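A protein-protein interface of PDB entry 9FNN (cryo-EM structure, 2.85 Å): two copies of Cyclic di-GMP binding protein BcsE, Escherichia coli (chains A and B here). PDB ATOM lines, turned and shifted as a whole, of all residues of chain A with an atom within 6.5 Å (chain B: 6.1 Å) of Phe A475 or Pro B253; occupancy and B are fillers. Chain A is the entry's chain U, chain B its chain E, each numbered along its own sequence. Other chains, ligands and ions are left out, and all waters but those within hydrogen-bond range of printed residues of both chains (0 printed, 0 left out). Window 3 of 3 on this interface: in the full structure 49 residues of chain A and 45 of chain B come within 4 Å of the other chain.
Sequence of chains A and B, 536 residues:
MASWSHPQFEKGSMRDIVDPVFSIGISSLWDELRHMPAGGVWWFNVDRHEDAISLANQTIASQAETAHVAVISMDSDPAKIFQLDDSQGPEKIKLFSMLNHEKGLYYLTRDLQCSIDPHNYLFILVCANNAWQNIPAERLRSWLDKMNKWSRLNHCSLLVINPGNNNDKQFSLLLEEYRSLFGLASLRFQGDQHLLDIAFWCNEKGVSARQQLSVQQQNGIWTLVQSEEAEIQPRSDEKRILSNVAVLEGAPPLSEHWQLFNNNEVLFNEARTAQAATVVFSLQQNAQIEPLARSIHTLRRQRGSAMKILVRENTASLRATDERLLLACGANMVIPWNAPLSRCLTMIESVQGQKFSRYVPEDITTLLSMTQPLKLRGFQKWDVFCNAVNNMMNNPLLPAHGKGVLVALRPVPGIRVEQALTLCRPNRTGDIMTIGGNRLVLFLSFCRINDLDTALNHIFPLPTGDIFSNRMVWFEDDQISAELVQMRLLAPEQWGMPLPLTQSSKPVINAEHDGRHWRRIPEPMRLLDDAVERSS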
ATOM      1  N   MET A 393      27.451  34.029  15.409  1.00  0.00           N
ATOM      2  CA  MET A 393      27.731  33.353  14.146  1.00  0.00           C
ATOM      3  C   MET A 393      29.219  33.122  13.925  1.00  0.00           C
ATOM      4  O   MET A 393      29.583  32.295  13.083  1.00  0.00           O
ATOM      5  CB  MET A 393      27.158  34.147  12.971  1.00  0.00           C
ATOM      6  CG  MET A 393      25.664  34.392  13.047  1.00  0.00           C
ATOM      7  SD  MET A 393      24.700  32.905  13.365  1.00  0.00           S
ATOM      8  CE  MET A 393      25.026  31.972  11.878  1.00  0.00           C
ATOM      9  N   HIS A 401      25.149  25.753  10.741  1.00  0.00           N
ATOM     10  CA  HIS A 401      23.777  25.841  10.245  1.00  0.00           C
ATOM     11  C   HIS A 401      22.768  25.382  11.292  1.00  0.00           C
ATOM     12  O   HIS A 401      21.711  24.842  10.958  1.00  0.00           O
ATOM     13  CB  HIS A 401      23.601  25.050   8.946  1.00  0.00           C
ATOM     14  CG  HIS A 401      24.534  25.469   7.854  1.00  0.00           C
ATOM     15  ND1 HIS A 401      25.891  25.240   7.905  1.00  0.00           N
ATOM     16  CD2 HIS A 401      24.304  26.104   6.680  1.00  0.00           C
ATOM     17  CE1 HIS A 401      26.457  25.716   6.811  1.00  0.00           C
ATOM     18  NE2 HIS A 401      25.517  26.244   6.051  1.00  0.00           N
ATOM     19  N   GLY A 402      23.088  25.590  12.565  1.00  0.00           N
ATOM     20  CA  GLY A 402      22.183  25.251  13.644  1.00  0.00           C
ATOM     21  C   GLY A 402      22.246  26.258  14.771  1.00  0.00           C
ATOM     22  O   GLY A 402      21.820  25.976  15.895  1.00  0.00           O
ATOM     23  N   LYS A 403      22.780  27.443  14.477  1.00  0.00           N
ATOM     24  CA  LYS A 403      22.963  28.459  15.503  1.00  0.00           C
ATOM     25  C   LYS A 403      21.665  29.170  15.863  1.00  0.00           C
ATOM     26  O   LYS A 403      21.485  29.562  17.020  1.00  0.00           O
ATOM     27  CB  LYS A 403      24.016  29.465  15.048  1.00  0.00           C
ATOM     28  CG  LYS A 403      25.355  28.828  14.739  1.00  0.00           C
ATOM     29  CD  LYS A 403      26.424  29.868  14.495  1.00  0.00           C
ATOM     30  CE  LYS A 403      27.739  29.218  14.113  1.00  0.00           C
ATOM     31  NZ  LYS A 403      27.620  28.435  12.855  1.00  0.00           N
ATOM     32  N   GLY A 404      20.759  29.347  14.913  1.00  0.00           N
ATOM     33  CA  GLY A 404      19.486  29.967  15.212  1.00  0.00           C
ATOM     34  C   GLY A 404      18.777  30.401  13.945  1.00  0.00           C
ATOM     35  O   GLY A 404      19.196  30.087  12.833  1.00  0.00           O
ATOM     36  N   VAL A 405      17.687  31.137  14.150  1.00  0.00           N
ATOM     37  CA  VAL A 405      16.856  31.658  13.071  1.00  0.00           C
ATOM     38  C   VAL A 405      16.778  33.172  13.206  1.00  0.00           C
ATOM     39  O   VAL A 405      16.433  33.688  14.274  1.00  0.00           O
ATOM     40  CB  VAL A 405      15.447  31.038  13.089  1.00  0.00           C
ATOM     41  CG1 VAL A 405      14.497  31.866  12.258  1.00  0.00           C
ATOM     42  CG2 VAL A 405      15.488  29.618  12.569  1.00  0.00           C
ATOM     43  N   LEU A 406      17.096  33.876  12.124  1.00  0.00           N
ATOM     44  CA  LEU A 406      16.959  35.326  12.037  1.00  0.00           C
ATOM     45  C   LEU A 406      15.761  35.615  11.143  1.00  0.00           C
ATOM     46  O   LEU A 406      15.792  35.317   9.945  1.00  0.00           O
ATOM     47  CB  LEU A 406      18.232  35.960  11.479  1.00  0.00           C
ATOM     48  CG  LEU A 406      18.306  37.482  11.396  1.00  0.00           C
ATOM     49  CD1 LEU A 406      18.568  38.077  12.762  1.00  0.00           C
ATOM     50  CD2 LEU A 406      19.367  37.918  10.411  1.00  0.00           C
ATOM     51  N   CYS A 447      17.226  27.655  17.448  1.00  0.00           N
ATOM     52  CA  CYS A 447      15.895  27.340  16.954  1.00  0.00           C
ATOM     53  C   CYS A 447      16.010  26.839  15.524  1.00  0.00           C
ATOM     54  O   CYS A 447      16.641  27.489  14.686  1.00  0.00           O
ATOM     55  CB  CYS A 447      14.976  28.561  17.016  1.00  0.00           C
ATOM     56  SG  CYS A 447      13.325  28.277  16.359  1.00  0.00           S
ATOM     57  N   ARG A 448      15.417  25.684  15.253  1.00  0.00           N
ATOM     58  CA  ARG A 448      15.440  25.156  13.902  1.00  0.00           C
ATOM     59  C   ARG A 448      14.370  25.826  13.048  1.00  0.00           C
ATOM     60  O   ARG A 448      13.434  26.453  13.551  1.00  0.00           O
ATOM     61  CB  ARG A 448      15.243  23.642  13.907  1.00  0.00           C
ATOM     62  CG  ARG A 448      16.436  22.870  14.436  1.00  0.00           C
ATOM     63  CD  ARG A 448      16.298  21.390  14.146  1.00  0.00           C
ATOM     64  NE  ARG A 448      17.504  20.648  14.489  1.00  0.00           N
ATOM     65  CZ  ARG A 448      17.690  20.008  15.633  1.00  0.00           C
ATOM     66  NH1 ARG A 448      16.760  19.990  16.573  1.00  0.00           N
ATOM     67  NH2 ARG A 448      18.835  19.366  15.839  1.00  0.00           N
ATOM     68  N   ILE A 449      14.532  25.701  11.733  1.00  0.00           N
ATOM     69  CA  ILE A 449      13.587  26.322  10.813  1.00  0.00           C
ATOM     70  C   ILE A 449      12.235  25.621  10.874  1.00  0.00           C
ATOM     71  O   ILE A 449      11.183  26.264  10.782  1.00  0.00           O
ATOM     72  CB  ILE A 449      14.170  26.339   9.388  1.00  0.00           C
ATOM     73  CG1 ILE A 449      13.154  26.896   8.396  1.00  0.00           C
ATOM     74  CG2 ILE A 449      14.631  24.954   8.973  1.00  0.00           C
ATOM     75  CD1 ILE A 449      12.733  28.303   8.697  1.00  0.00           C
ATOM     76  N   VAL A 473      13.007  34.701   6.439  1.00  0.00           N
ATOM     77  CA  VAL A 473      13.701  33.836   7.381  1.00  0.00           C
ATOM     78  C   VAL A 473      15.085  33.513   6.843  1.00  0.00           C
ATOM     79  O   VAL A 473      15.243  33.178   5.663  1.00  0.00           O
ATOM     80  CB  VAL A 473      12.914  32.540   7.649  1.00  0.00           C
ATOM     81  CG1 VAL A 473      13.562  31.761   8.767  1.00  0.00           C
ATOM     82  CG2 VAL A 473      11.471  32.858   7.984  1.00  0.00           C
ATOM     83  N   TRP A 474      16.088  33.619   7.712  1.00  0.00           N
ATOM     84  CA  TRP A 474      17.453  33.214   7.407  1.00  0.00           C
ATOM     85  C   TRP A 474      17.920  32.274   8.506  1.00  0.00           C
ATOM     86  O   TRP A 474      17.947  32.656   9.679  1.00  0.00           O
ATOM     87  CB  TRP A 474      18.378  34.426   7.299  1.00  0.00           C
ATOM     88  CG  TRP A 474      17.921  35.424   6.294  1.00  0.00           C
ATOM     89  CD1 TRP A 474      18.090  35.361   4.946  1.00  0.00           C
ATOM     90  CD2 TRP A 474      17.215  36.640   6.553  1.00  0.00           C
ATOM     91  NE1 TRP A 474      17.532  36.461   4.348  1.00  0.00           N
ATOM     92  CE2 TRP A 474      16.987  37.263   5.315  1.00  0.00           C
ATOM     93  CE3 TRP A 474      16.750  37.263   7.714  1.00  0.00           C
ATOM     94  CZ2 TRP A 474      16.317  38.475   5.202  1.00  0.00           C
ATOM     95  CZ3 TRP A 474      16.085  38.464   7.600  1.00  0.00           C
ATOM     96  CH2 TRP A 474      15.876  39.058   6.355  1.00  0.00           C
ATOM     97  N   PHE A 475      18.283  31.047   8.129  1.00  0.00           N
ATOM     98  CA  PHE A 475      18.685  30.035   9.096  1.00  0.00           C
ATOM     99  C   PHE A 475      20.040  29.415   8.782  1.00  0.00           C
ATOM    100  O   PHE A 475      20.423  28.435   9.431  1.00  0.00           O
ATOM    101  CB  PHE A 475      17.622  28.935   9.199  1.00  0.00           C
ATOM    102  CG  PHE A 475      17.329  28.247   7.900  1.00  0.00           C
ATOM    103  CD1 PHE A 475      16.463  28.807   6.983  1.00  0.00           C
ATOM    104  CD2 PHE A 475      17.905  27.027   7.606  1.00  0.00           C
ATOM    105  CE1 PHE A 475      16.191  28.174   5.794  1.00  0.00           C
ATOM    106  CE2 PHE A 475      17.634  26.388   6.417  1.00  0.00           C
ATOM    107  CZ  PHE A 475      16.776  26.963   5.512  1.00  0.00           C
ATOM    108  N   GLU A 476      20.775  29.955   7.816  1.00  0.00           N
ATOM    109  CA  GLU A 476      22.091  29.456   7.453  1.00  0.00           C
ATOM    110  C   GLU A 476      23.133  30.532   7.717  1.00  0.00           C
ATOM    111  O   GLU A 476      22.839  31.729   7.657  1.00  0.00           O
ATOM    112  CB  GLU A 476      22.134  29.022   5.988  1.00  0.00           C
ATOM    113  CG  GLU A 476      21.119  27.951   5.636  1.00  0.00           C
ATOM    114  CD  GLU A 476      21.286  27.425   4.224  1.00  0.00           C
ATOM    115  OE1 GLU A 476      22.417  27.477   3.700  1.00  0.00           O
ATOM    116  OE2 GLU A 476      20.285  26.965   3.637  1.00  0.00           O
ATOM    117  N   ASP A 477      24.358  30.092   8.015  1.00  0.00           N
ATOM    118  CA  ASP A 477      25.392  31.021   8.458  1.00  0.00           C
ATOM    119  C   ASP A 477      25.714  32.058   7.390  1.00  0.00           C
ATOM    120  O   ASP A 477      25.837  33.251   7.694  1.00  0.00           O
ATOM    121  CB  ASP A 477      26.651  30.254   8.854  1.00  0.00           C
ATOM    122  CG  ASP A 477      26.400  29.268   9.973  1.00  0.00           C
ATOM    123  OD1 ASP A 477      25.224  29.069  10.336  1.00  0.00           O
ATOM    124  OD2 ASP A 477      27.380  28.693  10.491  1.00  0.00           O
ATOM    125  N   GLN A 479      23.744  33.041   4.877  1.00  0.00           N
ATOM    126  CA  GLN A 479      22.582  33.905   4.704  1.00  0.00           C
ATOM    127  C   GLN A 479      22.442  34.885   5.862  1.00  0.00           C
ATOM    128  O   GLN A 479      22.165  36.071   5.652  1.00  0.00           O
ATOM    129  CB  GLN A 479      21.321  33.058   4.569  1.00  0.00           C
ATOM    130  CG  GLN A 479      21.462  31.876   3.632  1.00  0.00           C
ATOM    131  CD  GLN A 479      21.557  32.286   2.179  1.00  0.00           C
ATOM    132  OE1 GLN A 479      21.158  33.388   1.805  1.00  0.00           O
ATOM    133  NE2 GLN A 479      22.089  31.398   1.349  1.00  0.00           N
ATOM    134  N   ILE A 480      22.634  34.404   7.092  1.00  0.00           N
ATOM    135  CA  ILE A 480      22.523  35.272   8.260  1.00  0.00           C
ATOM    136  C   ILE A 480      23.601  36.345   8.233  1.00  0.00           C
ATOM    137  O   ILE A 480      23.340  37.514   8.539  1.00  0.00           O
ATOM    138  CB  ILE A 480      22.581  34.440   9.553  1.00  0.00           C
ATOM    139  CG1 ILE A 480      21.285  33.653   9.738  1.00  0.00           C
ATOM    140  CG2 ILE A 480      22.839  35.326  10.754  1.00  0.00           C
ATOM    141  CD1 ILE A 480      21.230  32.865  11.024  1.00  0.00           C
ATOM    142  N   LEU B 248      12.109  14.539   5.904  1.00  0.00           N
ATOM    143  CA  LEU B 248      11.661  15.861   6.318  1.00  0.00           C
ATOM    144  C   LEU B 248      10.206  16.030   5.903  1.00  0.00           C
ATOM    145  O   LEU B 248       9.891  16.004   4.709  1.00  0.00           O
ATOM    146  CB  LEU B 248      12.527  16.945   5.685  1.00  0.00           C
ATOM    147  CG  LEU B 248      14.025  16.666   5.640  1.00  0.00           C
ATOM    148  CD1 LEU B 248      14.746  17.796   4.941  1.00  0.00           C
ATOM    149  CD2 LEU B 248      14.564  16.468   7.043  1.00  0.00           C
ATOM    150  N   ALA B 251       9.808  20.137   5.622  1.00  0.00           N
ATOM    151  CA  ALA B 251      10.792  21.124   6.019  1.00  0.00           C
ATOM    152  C   ALA B 251      11.834  21.302   4.917  1.00  0.00           C
ATOM    153  O   ALA B 251      12.181  20.346   4.219  1.00  0.00           O
ATOM    154  CB  ALA B 251      11.475  20.708   7.318  1.00  0.00           C
ATOM    155  N   PRO B 252      12.340  22.516   4.737  1.00  0.00           N
ATOM    156  CA  PRO B 252      13.341  22.756   3.700  1.00  0.00           C
ATOM    157  C   PRO B 252      14.639  22.045   4.030  1.00  0.00           C
ATOM    158  O   PRO B 252      14.882  21.698   5.195  1.00  0.00           O
ATOM    159  CB  PRO B 252      13.522  24.282   3.728  1.00  0.00           C
ATOM    160  CG  PRO B 252      12.324  24.807   4.445  1.00  0.00           C
ATOM    161  CD  PRO B 252      11.959  23.754   5.432  1.00  0.00           C
ATOM    162  N   PRO B 253      15.476  21.770   3.024  1.00  0.00           N
ATOM    163  CA  PRO B 253      16.832  21.283   3.302  1.00  0.00           C
ATOM    164  C   PRO B 253      17.519  22.106   4.378  1.00  0.00           C
ATOM    165  O   PRO B 253      17.750  23.306   4.206  1.00  0.00           O
ATOM    166  CB  PRO B 253      17.539  21.424   1.951  1.00  0.00           C
ATOM    167  CG  PRO B 253      16.445  21.437   0.923  1.00  0.00           C
ATOM    168  CD  PRO B 253      15.116  21.618   1.606  1.00  0.00           C
ATOM    169  N   LEU B 254      17.845  21.461   5.498  1.00  0.00           N
ATOM    170  CA  LEU B 254      18.323  22.180   6.671  1.00  0.00           C
ATOM    171  C   LEU B 254      19.687  22.818   6.462  1.00  0.00           C
ATOM    172  O   LEU B 254      20.065  23.698   7.241  1.00  0.00           O
ATOM    173  CB  LEU B 254      18.382  21.244   7.878  1.00  0.00           C
ATOM    174  CG  LEU B 254      17.080  20.614   8.382  1.00  0.00           C
ATOM    175  CD1 LEU B 254      15.929  21.598   8.302  1.00  0.00           C
ATOM    176  CD2 LEU B 254      16.754  19.328   7.641  1.00  0.00           C
ATOM    177  N   SER B 255      20.435  22.408   5.443  1.00  0.00           N
ATOM    178  CA  SER B 255      21.779  22.929   5.251  1.00  0.00           C
ATOM    179  C   SER B 255      22.170  22.766   3.789  1.00  0.00           C
ATOM    180  O   SER B 255      21.390  22.288   2.962  1.00  0.00           O
ATOM    181  CB  SER B 255      22.778  22.229   6.173  1.00  0.00           C
ATOM    182  OG  SER B 255      24.094  22.699   5.945  1.00  0.00           O
ATOM    183  N   GLU B 256      23.396  23.188   3.479  1.00  0.00           N
ATOM    184  CA  GLU B 256      23.933  23.021   2.135  1.00  0.00           C
ATOM    185  C   GLU B 256      24.255  21.562   1.840  1.00  0.00           C
ATOM    186  O   GLU B 256      24.180  21.132   0.684  1.00  0.00           O
ATOM    187  CB  GLU B 256      25.179  23.890   1.973  1.00  0.00           C
ATOM    188  CG  GLU B 256      25.910  23.723   0.656  1.00  0.00           C
ATOM    189  CD  GLU B 256      27.279  24.372   0.672  1.00  0.00           C
ATOM    190  OE1 GLU B 256      27.630  24.994   1.697  1.00  0.00           O
ATOM    191  OE2 GLU B 256      28.006  24.256  -0.336  1.00  0.00           O
ATOM    192  N   TRP B 258      22.706  18.853   2.314  1.00  0.00           N
ATOM    193  CA  TRP B 258      21.558  17.961   2.217  1.00  0.00           C
ATOM    194  C   TRP B 258      21.171  17.746   0.760  1.00  0.00           C
ATOM    195  O   TRP B 258      21.076  18.705  -0.012  1.00  0.00           O
ATOM    196  CB  TRP B 258      20.369  18.525   2.991  1.00  0.00           C
ATOM    197  CG  TRP B 258      20.416  18.262   4.455  1.00  0.00           C
ATOM    198  CD1 TRP B 258      21.272  18.812   5.357  1.00  0.00           C
ATOM    199  CD2 TRP B 258      19.556  17.394   5.195  1.00  0.00           C
ATOM    200  NE1 TRP B 258      21.005  18.334   6.615  1.00  0.00           N
ATOM    201  CE2 TRP B 258      19.954  17.460   6.541  1.00  0.00           C
ATOM    202  CE3 TRP B 258      18.490  16.562   4.850  1.00  0.00           C
ATOM    203  CZ2 TRP B 258      19.325  16.728   7.539  1.00  0.00           C
ATOM    204  CZ3 TRP B 258      17.869  15.837   5.841  1.00  0.00           C
ATOM    205  CH2 TRP B 258      18.285  15.924   7.169  1.00  0.00           C
ATOM    206  N   LEU B 260      18.047  15.553  -1.272  1.00  0.00           N
ATOM    207  CA  LEU B 260      16.791  14.848  -1.059  1.00  0.00           C
ATOM    208  C   LEU B 260      16.460  14.009  -2.284  1.00  0.00           C
ATOM    209  O   LEU B 260      16.518  14.501  -3.415  1.00  0.00           O
ATOM    210  CB  LEU B 260      15.651  15.825  -0.763  1.00  0.00           C
ATOM    211  CG  LEU B 260      15.576  16.438   0.637  1.00  0.00           C
ATOM    212  CD1 LEU B 260      15.712  15.366   1.701  1.00  0.00           C
ATOM    213  CD2 LEU B 260      16.618  17.532   0.831  1.00  0.00           C
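The side-chain carboxylate (OD1) of Asp A477 sits at hydrogen-bond distance from the backbone NH (N) of His A401.
Among the printed residues, pairs that only touch across the chains: His A401 with Ser B255, Ile A449 with Leu B254, Phe A475 with Leu B254 and Phe A475 with Pro B253.
Of the printed residues of chain B, Ile A449 touches Leu B254. Of chain A, only Phe A475 (3.8 Å) comes within 4 Å of Pro B253. Of the printed residues of chain A, Leu B254 touches Ile A449 and Phe A475. Of the printed residues of chain A, Ser B255 touches His A401 (3.4 Å). The nearest residue of chain B that does not touch Phe A475 is Pro B252 (4.6 Å).
Of the 17 printed residues of chain A, 3 touch a printed residue of chain B. Printed residues of chain A that touch a printed residue of chain B: His A401, Ile A449 and Phe A475. Hydrophobic or aromatic side chains of chain A that line the printed part of chain B: His A401, Ile A449 and Phe A475. Among the printed residues, no Asp or Glu carboxylate lies within 4 Å of a Lys or Arg side-chain nitrogen of the other chain.
No position is printed for both chains.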
